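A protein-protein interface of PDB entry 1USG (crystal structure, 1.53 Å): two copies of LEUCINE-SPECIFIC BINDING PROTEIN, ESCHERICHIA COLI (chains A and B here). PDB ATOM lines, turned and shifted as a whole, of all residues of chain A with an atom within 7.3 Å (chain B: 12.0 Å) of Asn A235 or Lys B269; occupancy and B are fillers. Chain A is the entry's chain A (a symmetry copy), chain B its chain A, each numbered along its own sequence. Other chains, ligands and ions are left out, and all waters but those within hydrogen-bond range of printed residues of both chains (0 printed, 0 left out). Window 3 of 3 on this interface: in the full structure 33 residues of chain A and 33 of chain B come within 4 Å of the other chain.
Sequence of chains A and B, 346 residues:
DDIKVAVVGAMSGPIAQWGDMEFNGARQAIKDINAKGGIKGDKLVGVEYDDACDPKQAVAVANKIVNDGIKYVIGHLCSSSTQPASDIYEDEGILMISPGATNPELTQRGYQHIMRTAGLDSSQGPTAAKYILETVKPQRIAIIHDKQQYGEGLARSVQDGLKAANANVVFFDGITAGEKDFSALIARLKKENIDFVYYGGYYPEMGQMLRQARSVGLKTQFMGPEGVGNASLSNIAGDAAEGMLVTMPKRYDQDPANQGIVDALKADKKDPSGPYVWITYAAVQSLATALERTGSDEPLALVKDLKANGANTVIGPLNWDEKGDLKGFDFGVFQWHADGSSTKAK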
ATOM      1  N   ASN A 230      -0.396  17.012  22.271  1.00  0.00           N
ATOM      2  CA  ASN A 230       0.912  17.519  22.723  1.00  0.00           C
ATOM      3  C   ASN A 230       2.012  17.194  21.714  1.00  0.00           C
ATOM      4  O   ASN A 230       1.969  16.157  21.059  1.00  0.00           O
ATOM      5  CB  ASN A 230       1.212  16.903  24.090  1.00  0.00           C
ATOM      6  CG  ASN A 230       2.382  17.544  24.797  1.00  0.00           C
ATOM      7  OD1 ASN A 230       3.525  17.262  24.502  1.00  0.00           O
ATOM      8  ND2 ASN A 230       2.088  18.373  25.784  1.00  0.00           N
ATOM      9  N   ALA A 231       3.001  18.070  21.587  1.00  0.00           N
ATOM     10  CA  ALA A 231       4.012  17.881  20.548  1.00  0.00           C
ATOM     11  C   ALA A 231       4.899  16.666  20.844  1.00  0.00           C
ATOM     12  O   ALA A 231       5.579  16.165  19.929  1.00  0.00           O
ATOM     13  CB  ALA A 231       4.852  19.142  20.373  1.00  0.00           C
ATOM     14  N   SER A 232       4.877  16.182  22.084  1.00  0.00           N
ATOM     15  CA  SER A 232       5.630  14.985  22.466  1.00  0.00           C
ATOM     16  C   SER A 232       4.773  13.685  22.370  1.00  0.00           C
ATOM     17  O   SER A 232       5.260  12.577  22.643  1.00  0.00           O
ATOM     18  CB  SER A 232       6.340  15.181  23.835  1.00  0.00           C
ATOM     19  OG  SER A 232       5.473  15.077  24.959  1.00  0.00           O
ATOM     20  N   LEU A 233       3.518  13.826  21.930  1.00  0.00           N
ATOM     21  CA  LEU A 233       2.627  12.690  21.686  1.00  0.00           C
ATOM     22  C   LEU A 233       3.150  11.869  20.538  1.00  0.00           C
ATOM     23  O   LEU A 233       3.423  10.675  20.688  1.00  0.00           O
ATOM     24  CB  LEU A 233       1.217  13.138  21.306  1.00  0.00           C
ATOM     25  CG  LEU A 233       0.314  12.028  20.751  1.00  0.00           C
ATOM     26  CD1 LEU A 233      -0.152  11.108  21.889  1.00  0.00           C
ATOM     27  CD2 LEU A 233      -0.851  12.614  20.012  1.00  0.00           C
ATOM     28  N   SER A 234       3.241  12.527  19.384  1.00  0.00           N
ATOM     29  CA  SER A 234       3.798  11.908  18.187  1.00  0.00           C
ATOM     30  C   SER A 234       5.220  11.455  18.452  1.00  0.00           C
ATOM     31  O   SER A 234       5.751  10.660  17.708  1.00  0.00           O
ATOM     32  CB  SER A 234       3.743  12.861  16.997  1.00  0.00           C
ATOM     33  OG  SER A 234       2.393  13.134  16.624  1.00  0.00           O
ATOM     34  N   ASN A 235       5.834  11.958  19.515  1.00  0.00           N
ATOM     35  CA  ASN A 235       7.127  11.427  19.970  1.00  0.00           C
ATOM     36  C   ASN A 235       7.103  10.004  20.565  1.00  0.00           C
ATOM     37  O   ASN A 235       7.986   9.187  20.278  1.00  0.00           O
ATOM     38  CB  ASN A 235       7.761  12.398  20.970  1.00  0.00           C
ATOM     39  CG  ASN A 235       9.238  12.560  20.751  1.00  0.00           C
ATOM     40  OD1 ASN A 235       9.673  12.940  19.660  1.00  0.00           O
ATOM     41  ND2 ASN A 235      10.028  12.218  21.757  1.00  0.00           N
ATOM     42  N   ILE A 236       6.092   9.723  21.394  1.00  0.00           N
ATOM     43  CA  ILE A 236       5.833   8.426  22.018  1.00  0.00           C
ATOM     44  C   ILE A 236       5.199   7.450  21.017  1.00  0.00           C
ATOM     45  O   ILE A 236       5.490   6.246  21.020  1.00  0.00           O
ATOM     46  CB  ILE A 236       4.790   8.621  23.188  1.00  0.00           C
ATOM     47  CG1 ILE A 236       5.387   9.433  24.335  1.00  0.00           C
ATOM     48  CG2 ILE A 236       4.272   7.280  23.730  1.00  0.00           C
ATOM     49  CD1 ILE A 236       4.333  10.177  25.139  1.00  0.00           C
ATOM     50  N   ALA A 237       4.304   7.969  20.198  1.00  0.00           N
ATOM     51  CA  ALA A 237       3.453   7.134  19.371  1.00  0.00           C
ATOM     52  C   ALA A 237       3.978   6.965  17.956  1.00  0.00           C
ATOM     53  O   ALA A 237       3.609   6.020  17.266  1.00  0.00           O
ATOM     54  CB  ALA A 237       2.048   7.709  19.344  1.00  0.00           C
ATOM     55  N   GLY A 238       4.822   7.904  17.530  1.00  0.00           N
ATOM     56  CA  GLY A 238       5.297   7.989  16.162  1.00  0.00           C
ATOM     57  C   GLY A 238       4.181   8.137  15.169  1.00  0.00           C
ATOM     58  O   GLY A 238       3.225   8.913  15.349  1.00  0.00           O
ATOM     59  N   ASP A 239       4.301   7.386  14.091  1.00  0.00           N
ATOM     60  CA  ASP A 239       3.347   7.433  13.010  1.00  0.00           C
ATOM     61  C   ASP A 239       1.929   7.080  13.508  1.00  0.00           C
ATOM     62  O   ASP A 239       0.945   7.414  12.839  1.00  0.00           O
ATOM     63  CB  ASP A 239       3.757   6.451  11.889  1.00  0.00           C
ATOM     64  CG  ASP A 239       4.879   7.001  10.968  1.00  0.00           C
ATOM     65  OD1 ASP A 239       5.245   8.198  11.051  1.00  0.00           O
ATOM     66  OD2 ASP A 239       5.450   6.284  10.108  1.00  0.00           O
ATOM     67  N   ALA A 241       0.128   8.289  15.791  1.00  0.00           N
ATOM     68  CA  ALA A 241      -0.740   9.420  16.101  1.00  0.00           C
ATOM     69  C   ALA A 241      -1.467   9.957  14.863  1.00  0.00           C
ATOM     70  O   ALA A 241      -2.388  10.748  14.949  1.00  0.00           O
ATOM     71  CB  ALA A 241       0.046  10.524  16.748  1.00  0.00           C
ATOM     72  N   TRP A 336      -4.890  15.007  14.010  1.00  0.00           N
ATOM     73  CA  TRP A 336      -3.482  15.039  14.324  1.00  0.00           C
ATOM     74  C   TRP A 336      -2.662  14.358  13.234  1.00  0.00           C
ATOM     75  O   TRP A 336      -3.125  13.440  12.579  1.00  0.00           O
ATOM     76  CB  TRP A 336      -3.215  14.318  15.662  1.00  0.00           C
ATOM     77  CG  TRP A 336      -2.030  14.834  16.415  1.00  0.00           C
ATOM     78  CD1 TRP A 336      -0.771  14.299  16.452  1.00  0.00           C
ATOM     79  CD2 TRP A 336      -1.984  15.996  17.238  1.00  0.00           C
ATOM     80  NE1 TRP A 336       0.041  15.049  17.269  1.00  0.00           N
ATOM     81  CE2 TRP A 336      -0.674  16.109  17.748  1.00  0.00           C
ATOM     82  CE3 TRP A 336      -2.918  16.964  17.583  1.00  0.00           C
ATOM     83  CZ2 TRP A 336      -0.296  17.141  18.611  1.00  0.00           C
ATOM     84  CZ3 TRP A 336      -2.537  17.993  18.438  1.00  0.00           C
ATOM     85  CH2 TRP A 336      -1.239  18.080  18.918  1.00  0.00           C
ATOM     86  N   ALA A 338       1.446  12.721  12.215  1.00  0.00           N
ATOM     87  CA  ALA A 338       2.691  12.162  12.727  1.00  0.00           C
ATOM     88  C   ALA A 338       3.758  13.206  13.052  1.00  0.00           C
ATOM     89  O   ALA A 338       4.581  12.983  13.937  1.00  0.00           O
ATOM     90  CB  ALA A 338       3.228  11.152  11.759  1.00  0.00           C
ATOM     91  N   ASP A 339       3.742  14.346  12.362  1.00  0.00           N
ATOM     92  CA  ASP A 339       4.757  15.373  12.601  1.00  0.00           C
ATOM     93  C   ASP A 339       4.371  16.393  13.675  1.00  0.00           C
ATOM     94  O   ASP A 339       5.077  17.372  13.881  1.00  0.00           O
ATOM     95  CB  ASP A 339       5.143  16.078  11.289  1.00  0.00           C
ATOM     96  CG  ASP A 339       4.018  16.924  10.721  1.00  0.00           C
ATOM     97  OD1 ASP A 339       2.924  16.932  11.314  1.00  0.00           O
ATOM     98  OD2 ASP A 339       4.118  17.618   9.686  1.00  0.00           O
ATOM     99  N   GLY A 340       3.258  16.157  14.370  1.00  0.00           N
ATOM    100  CA  GLY A 340       2.822  17.026  15.447  1.00  0.00           C
ATOM    101  C   GLY A 340       1.915  18.159  15.011  1.00  0.00           C
ATOM    102  O   GLY A 340       1.325  18.861  15.843  1.00  0.00           O
ATOM    103  N   GLN B  17      -0.668  25.381  27.965  1.00  0.00           N
ATOM    104  CA  GLN B  17       0.558  25.641  27.234  1.00  0.00           C
ATOM    105  C   GLN B  17       1.686  26.058  28.166  1.00  0.00           C
ATOM    106  O   GLN B  17       2.835  25.603  28.026  1.00  0.00           O
ATOM    107  CB  GLN B  17       0.352  26.688  26.130  1.00  0.00           C
ATOM    108  CG  GLN B  17      -0.615  26.188  25.079  1.00  0.00           C
ATOM    109  CD  GLN B  17      -0.677  27.053  23.817  1.00  0.00           C
ATOM    110  OE1 GLN B  17      -0.331  28.243  23.842  1.00  0.00           O
ATOM    111  NE2 GLN B  17      -1.119  26.448  22.708  1.00  0.00           N
ATOM    112  N   ASP B  20       2.694  23.000  30.227  1.00  0.00           N
ATOM    113  CA  ASP B  20       3.635  22.110  29.523  1.00  0.00           C
ATOM    114  C   ASP B  20       5.078  22.587  29.666  1.00  0.00           C
ATOM    115  O   ASP B  20       5.961  21.799  29.880  1.00  0.00           O
ATOM    116  CB  ASP B  20       3.247  22.005  28.037  1.00  0.00           C
ATOM    117  CG  ASP B  20       3.970  20.907  27.302  1.00  0.00           C
ATOM    118  OD1 ASP B  20       3.758  19.728  27.618  1.00  0.00           O
ATOM    119  OD2 ASP B  20       4.788  21.166  26.394  1.00  0.00           O
ATOM    120  N   MET B  21       5.301  23.887  29.593  1.00  0.00           N
ATOM    121  CA  MET B  21       6.609  24.499  29.815  1.00  0.00           C
ATOM    122  C   MET B  21       7.152  24.109  31.212  1.00  0.00           C
ATOM    123  O   MET B  21       8.276  23.626  31.380  1.00  0.00           O
ATOM    124  CB  MET B  21       6.534  26.010  29.748  1.00  0.00           C
ATOM    125  CG  MET B  21       6.136  26.548  28.437  1.00  0.00           C
ATOM    126  SD  MET B  21       5.978  28.335  28.595  1.00  0.00           S
ATOM    127  CE  MET B  21       5.304  28.740  26.985  1.00  0.00           C
ATOM    128  N   PHE B  23       6.176  21.541  33.263  1.00  0.00           N
ATOM    129  CA  PHE B  23       6.471  20.106  33.421  1.00  0.00           C
ATOM    130  C   PHE B  23       7.729  19.757  32.619  1.00  0.00           C
ATOM    131  O   PHE B  23       8.543  18.989  33.077  1.00  0.00           O
ATOM    132  CB  PHE B  23       5.289  19.266  32.945  1.00  0.00           C
ATOM    133  CG  PHE B  23       4.091  19.346  33.845  1.00  0.00           C
ATOM    134  CD1 PHE B  23       2.895  19.905  33.394  1.00  0.00           C
ATOM    135  CD2 PHE B  23       4.153  18.926  35.159  1.00  0.00           C
ATOM    136  CE1 PHE B  23       1.805  20.016  34.171  1.00  0.00           C
ATOM    137  CE2 PHE B  23       3.028  19.009  35.955  1.00  0.00           C
ATOM    138  CZ  PHE B  23       1.854  19.589  35.465  1.00  0.00           C
ATOM    139  N   ASN B  24       7.917  20.330  31.446  1.00  0.00           N
ATOM    140  CA  ASN B  24       9.134  20.036  30.667  1.00  0.00           C
ATOM    141  C   ASN B  24      10.409  20.492  31.394  1.00  0.00           C
ATOM    142  O   ASN B  24      11.448  19.803  31.387  1.00  0.00           O
ATOM    143  CB  ASN B  24       9.065  20.715  29.291  1.00  0.00           C
ATOM    144  CG  ASN B  24       8.055  20.062  28.364  1.00  0.00           C
ATOM    145  OD1 ASN B  24       7.622  18.953  28.597  1.00  0.00           O
ATOM    146  ND2 ASN B  24       7.669  20.794  27.296  1.00  0.00           N
ATOM    147  N   GLY B  25      10.387  21.691  31.992  1.00  0.00           N
ATOM    148  CA  GLY B  25      11.540  22.200  32.689  1.00  0.00           C
ATOM    149  C   GLY B  25      11.821  21.355  33.928  1.00  0.00           C
ATOM    150  O   GLY B  25      12.962  21.030  34.193  1.00  0.00           O
ATOM    151  N   ARG B  27      10.999  18.184  34.460  1.00  0.00           N
ATOM    152  CA  ARG B  27      11.418  16.838  34.046  1.00  0.00           C
ATOM    153  C   ARG B  27      12.896  16.884  33.642  1.00  0.00           C
ATOM    154  O   ARG B  27      13.703  16.001  34.006  1.00  0.00           O
ATOM    155  CB  ARG B  27      10.568  16.357  32.878  1.00  0.00           C
ATOM    156  CG  ARG B  27       9.204  15.859  33.196  1.00  0.00           C
ATOM    157  CD  ARG B  27       8.417  15.442  31.901  1.00  0.00           C
ATOM    158  NE  ARG B  27       6.971  15.513  32.101  1.00  0.00           N
ATOM    159  CZ  ARG B  27       6.110  15.986  31.213  1.00  0.00           C
ATOM    160  NH1 ARG B  27       6.539  16.405  30.040  1.00  0.00           N
ATOM    161  NH2 ARG B  27       4.804  15.996  31.492  1.00  0.00           N
ATOM    162  N   GLN B  28      13.275  17.878  32.841  1.00  0.00           N
ATOM    163  CA  GLN B  28      14.661  17.946  32.384  1.00  0.00           C
ATOM    164  C   GLN B  28      15.618  18.182  33.538  1.00  0.00           C
ATOM    165  O   GLN B  28      16.702  17.633  33.595  1.00  0.00           O
ATOM    166  CB  GLN B  28      14.834  18.981  31.278  1.00  0.00           C
ATOM    167  CG  GLN B  28      16.151  18.858  30.528  1.00  0.00           C
ATOM    168  CD  GLN B  28      16.319  17.499  29.824  1.00  0.00           C
ATOM    169  OE1 GLN B  28      15.417  17.011  29.127  1.00  0.00           O
ATOM    170  NE2 GLN B  28      17.508  16.897  30.006  1.00  0.00           N
ATOM    171  N   LYS B  31      16.133  14.937  35.485  1.00  0.00           N
ATOM    172  CA  LYS B  31      16.995  14.033  34.720  1.00  0.00           C
ATOM    173  C   LYS B  31      18.442  14.514  34.817  1.00  0.00           C
ATOM    174  O   LYS B  31      19.362  13.708  35.062  1.00  0.00           O
ATOM    175  CB  LYS B  31      16.509  13.972  33.257  1.00  0.00           C
ATOM    176  CG  LYS B  31      17.256  13.016  32.393  1.00  0.00           C
ATOM    177  CD  LYS B  31      16.521  12.829  31.075  1.00  0.00           C
ATOM    178  CE  LYS B  31      17.398  12.259  30.007  1.00  0.00           C
ATOM    179  NZ  LYS B  31      16.567  12.076  28.780  1.00  0.00           N
ATOM    180  N   GLY B 260      22.688  23.016  26.365  1.00  0.00           N
ATOM    181  CA  GLY B 260      22.491  21.599  26.573  1.00  0.00           C
ATOM    182  C   GLY B 260      21.031  21.285  26.834  1.00  0.00           C
ATOM    183  O   GLY B 260      20.442  20.317  26.335  1.00  0.00           O
ATOM    184  N   ILE B 261      20.426  22.164  27.619  1.00  0.00           N
ATOM    185  CA  ILE B 261      19.030  22.025  27.974  1.00  0.00           C
ATOM    186  C   ILE B 261      18.154  22.364  26.762  1.00  0.00           C
ATOM    187  O   ILE B 261      17.184  21.683  26.471  1.00  0.00           O
ATOM    188  CB  ILE B 261      18.725  22.929  29.200  1.00  0.00           C
ATOM    189  CG1 ILE B 261      19.532  22.466  30.432  1.00  0.00           C
ATOM    190  CG2 ILE B 261      17.205  22.918  29.521  1.00  0.00           C
ATOM    191  CD1 ILE B 261      19.693  23.482  31.520  1.00  0.00           C
ATOM    192  N   VAL B 262      18.507  23.427  26.061  1.00  0.00           N
ATOM    193  CA  VAL B 262      17.824  23.775  24.820  1.00  0.00           C
ATOM    194  C   VAL B 262      17.831  22.587  23.842  1.00  0.00           C
ATOM    195  O   VAL B 262      16.810  22.297  23.229  1.00  0.00           O
ATOM    196  CB  VAL B 262      18.461  25.027  24.155  1.00  0.00           C
ATOM    197  CG1 VAL B 262      17.876  25.278  22.790  1.00  0.00           C
ATOM    198  CG2 VAL B 262      18.287  26.295  25.009  1.00  0.00           C
ATOM    199  N   ASP B 263      18.937  21.840  23.789  1.00  0.00           N
ATOM    200  CA  ASP B 263      19.070  20.692  22.874  1.00  0.00           C
ATOM    201  C   ASP B 263      18.255  19.491  23.287  1.00  0.00           C
ATOM    202  O   ASP B 263      17.637  18.810  22.462  1.00  0.00           O
ATOM    203  CB  ASP B 263      20.547  20.301  22.787  1.00  0.00           C
ATOM    204  CG  ASP B 263      21.392  21.404  22.185  1.00  0.00           C
ATOM    205  OD1 ASP B 263      22.623  21.468  22.433  1.00  0.00           O
ATOM    206  OD2 ASP B 263      20.901  22.266  21.425  1.00  0.00           O
ATOM    207  N   ALA B 264      18.234  19.226  24.597  1.00  0.00           N
ATOM    208  CA  ALA B 264      17.434  18.149  25.128  1.00  0.00           C
ATOM    209  C   ALA B 264      15.985  18.409  24.855  1.00  0.00           C
ATOM    210  O   ALA B 264      15.237  17.488  24.501  1.00  0.00           O
ATOM    211  CB  ALA B 264      17.685  17.984  26.632  1.00  0.00           C
ATOM    212  N   LEU B 265      15.567  19.669  25.049  1.00  0.00           N
ATOM    213  CA  LEU B 265      14.187  20.051  24.809  1.00  0.00           C
ATOM    214  C   LEU B 265      13.840  19.872  23.335  1.00  0.00           C
ATOM    215  O   LEU B 265      12.863  19.184  23.029  1.00  0.00           O
ATOM    216  CB  LEU B 265      13.905  21.478  25.313  1.00  0.00           C
ATOM    217  CG  LEU B 265      13.958  21.586  26.854  1.00  0.00           C
ATOM    218  CD1 LEU B 265      14.127  23.033  27.315  1.00  0.00           C
ATOM    219  CD2 LEU B 265      12.731  20.952  27.484  1.00  0.00           C
ATOM    220  N   LYS B 266      14.633  20.473  22.450  1.00  0.00           N
ATOM    221  CA  LYS B 266      14.380  20.395  20.997  1.00  0.00           C
ATOM    222  C   LYS B 266      14.384  18.933  20.519  1.00  0.00           C
ATOM    223  O   LYS B 266      13.529  18.518  19.726  1.00  0.00           O
ATOM    224  CB  LYS B 266      15.414  21.232  20.230  1.00  0.00           C
ATOM    225  CG  LYS B 266      15.144  22.732  20.230  1.00  0.00           C
ATOM    226  CD  LYS B 266      15.913  23.452  19.149  1.00  0.00           C
ATOM    227  CE  LYS B 266      16.871  24.480  19.724  1.00  0.00           C
ATOM    228  NZ  LYS B 266      17.175  25.577  18.723  1.00  0.00           N
ATOM    229  N   ALA B 267      15.319  18.137  21.022  1.00  0.00           N
ATOM    230  CA  ALA B 267      15.334  16.702  20.702  1.00  0.00           C
ATOM    231  C   ALA B 267      14.021  15.976  21.067  1.00  0.00           C
ATOM    232  O   ALA B 267      13.617  15.050  20.362  1.00  0.00           O
ATOM    233  CB  ALA B 267      16.527  16.024  21.370  1.00  0.00           C
ATOM    234  N   ASP B 268      13.355  16.399  22.150  1.00  0.00           N
ATOM    235  CA  ASP B 268      12.082  15.800  22.580  1.00  0.00           C
ATOM    236  C   ASP B 268      10.876  16.519  21.951  1.00  0.00           C
ATOM    237  O   ASP B 268       9.727  16.281  22.342  1.00  0.00           O
ATOM    238  CB  ASP B 268      11.936  15.823  24.116  1.00  0.00           C
ATOM    239  CG  ASP B 268      13.008  14.998  24.840  1.00  0.00           C
ATOM    240  OD1 ASP B 268      13.440  13.941  24.311  1.00  0.00           O
ATOM    241  OD2 ASP B 268      13.466  15.334  25.965  1.00  0.00           O
ATOM    242  N   LYS B 269      11.159  17.375  20.969  1.00  0.00           N
ATOM    243  CA  LYS B 269      10.185  18.226  20.271  1.00  0.00           C
ATOM    244  C   LYS B 269       9.456  19.198  21.191  1.00  0.00           C
ATOM    245  O   LYS B 269       8.263  19.458  21.030  1.00  0.00           O
ATOM    246  CB  LYS B 269       9.181  17.392  19.465  1.00  0.00           C
ATOM    247  CG  LYS B 269       9.707  16.988  18.085  1.00  0.00           C
ATOM    248  CD  LYS B 269      10.061  15.516  18.105  1.00  0.00           C
ATOM    249  CE  LYS B 269      10.501  14.997  16.729  1.00  0.00           C
ATOM    250  NZ  LYS B 269      10.828  13.528  16.814  1.00  0.00           N
ATOM    251  N   LYS B 270      10.190  19.747  22.149  1.00  0.00           N
ATOM    252  CA  LYS B 270       9.625  20.710  23.081  1.00  0.00           C
ATOM    253  C   LYS B 270      10.227  22.085  22.831  1.00  0.00           C
ATOM    254  O   LYS B 270      11.429  22.237  22.590  1.00  0.00           O
ATOM    255  CB  LYS B 270       9.833  20.232  24.523  1.00  0.00           C
ATOM    256  CG  LYS B 270       9.252  18.841  24.788  1.00  0.00           C
ATOM    257  CD  LYS B 270       9.761  18.186  26.072  1.00  0.00           C
ATOM    258  CE  LYS B 270       9.080  16.840  26.305  1.00  0.00           C
ATOM    259  NZ  LYS B 270       9.538  16.169  27.539  1.00  0.00           N
ATOM    260  N   ASP B 271       9.366  23.091  22.817  1.00  0.00           N
ATOM    261  CA  ASP B 271       9.793  24.459  22.653  1.00  0.00           C
ATOM    262  C   ASP B 271      10.566  24.938  23.901  1.00  0.00           C
ATOM    263  O   ASP B 271      10.023  24.925  25.010  1.00  0.00           O
ATOM    264  CB  ASP B 271       8.573  25.336  22.419  1.00  0.00           C
ATOM    265  CG  ASP B 271       8.938  26.733  22.020  1.00  0.00           C
ATOM    266  OD1 ASP B 271       8.065  27.423  21.484  1.00  0.00           O
ATOM    267  OD2 ASP B 271      10.062  27.251  22.198  1.00  0.00           O
ATOM    268  N   PRO B 272      11.825  25.320  23.722  1.00  0.00           N
ATOM    269  CA  PRO B 272      12.650  25.826  24.825  1.00  0.00           C
ATOM    270  C   PRO B 272      12.528  27.326  25.086  1.00  0.00           C
ATOM    271  O   PRO B 272      13.236  27.823  25.958  1.00  0.00           O
ATOM    272  CB  PRO B 272      14.072  25.542  24.340  1.00  0.00           C
ATOM    273  CG  PRO B 272      13.993  25.752  22.889  1.00  0.00           C
ATOM    274  CD  PRO B 272      12.601  25.235  22.465  1.00  0.00           C
ATOM    275  N   SER B 273      11.684  28.049  24.346  1.00  0.00           N
ATOM    276  CA  SER B 273      11.650  29.497  24.478  1.00  0.00           C
ATOM    277  C   SER B 273      10.852  29.991  25.655  1.00  0.00           C
ATOM    278  O   SER B 273      10.962  31.145  26.053  1.00  0.00           O
ATOM    279  CB  SER B 273      11.065  30.170  23.225  1.00  0.00           C
ATOM    280  OG  SER B 273       9.780  29.678  22.948  1.00  0.00           O
ATOM    281  N   GLY B 274      10.002  29.126  26.188  1.00  0.00           N
ATOM    282  CA  GLY B 274       9.024  29.565  27.162  1.00  0.00           C
ATOM    283  C   GLY B 274       9.648  29.871  28.516  1.00  0.00           C
ATOM    284  O   GLY B 274      10.417  29.055  29.000  1.00  0.00           O
ATOM    285  N   VAL B 277       9.723  27.228  31.382  1.00  0.00           N
ATOM    286  CA  VAL B 277      10.670  26.132  31.348  1.00  0.00           C
ATOM    287  C   VAL B 277      11.818  26.397  32.321  1.00  0.00           C
ATOM    288  O   VAL B 277      12.173  25.552  33.180  1.00  0.00           O
ATOM    289  CB  VAL B 277      11.259  25.986  29.952  1.00  0.00           C
ATOM    290  CG1 VAL B 277      12.335  24.925  29.955  1.00  0.00           C
ATOM    291  CG2 VAL B 277      10.179  25.659  28.921  1.00  0.00           C
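Hydrophobic or aromatic side chains of chain A within 4 Å of the printed part of chain B: Ala A231. Among the printed residues, 4 pairs touch across the chains. Among the printed residues, no Asp or Glu carboxylate lies within 4 Å of a Lys or Arg side-chain nitrogen of the other chain.
Of the printed residues of chain B, Asn A230 touches Asp B20 (2.8 Å). Ala A231 touches one residue of chain B. Of the printed residues of chain B, Ser A232 touches Asp B268. No residue of chain B comes within 4 Å of Ser A234. Printed residues of chain B within 4 Å of Asn A235: Lys B269. No residue of chain B comes within 4 Å of Ala A237. No residue of chain B comes within 4 Å of Gly A238. Printed residues of chain A within 4 Å of Asp B20: Asn A230. Printed residues of chain A within 4 Å of Asp B268: Ser A232 (3.9 Å). Lys B269 touches just these residues of chain A: Ala A231 (3.5 Å) and Asn A235 (3.0 Å). Val B277 touches none of the printed residues of chain A. The nearest residue of chain A that does not touch Lys B269 is Ser A232 (4.8 Å). The nearest printed residue of chain B that does not touch Asn A230 is Lys B270 (5.9 Å).
No position is printed for both chains. Of the 4 pairs that touch across the chains among the printed residues, none has its exchanged pair printed and touching as well.
Among the printed residues, merely in contact across the chains: Ala A231 with Lys B269 (3.5 Å) and Ser A232 with Asp B268 (3.9 Å).
OD2 of Asp B20 lies within hydrogen-bond range of ND2 of Asn B24, 3.0 Å away. The side-chain hydroxyl (OG) of Ser A232 is in hydrogen-bond range of the side-chain amide oxygen (OD1) of Asn A230 (3.0 Å).
OD1 of Asp B20 is in hydrogen-bond range of ND2 of Asn A230, 2.8 Å away. The side-chain amino group (NZ) of Lys B269 lies close to the side-chain amide oxygen (OD1) of Asn A235 (3.1 Å).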
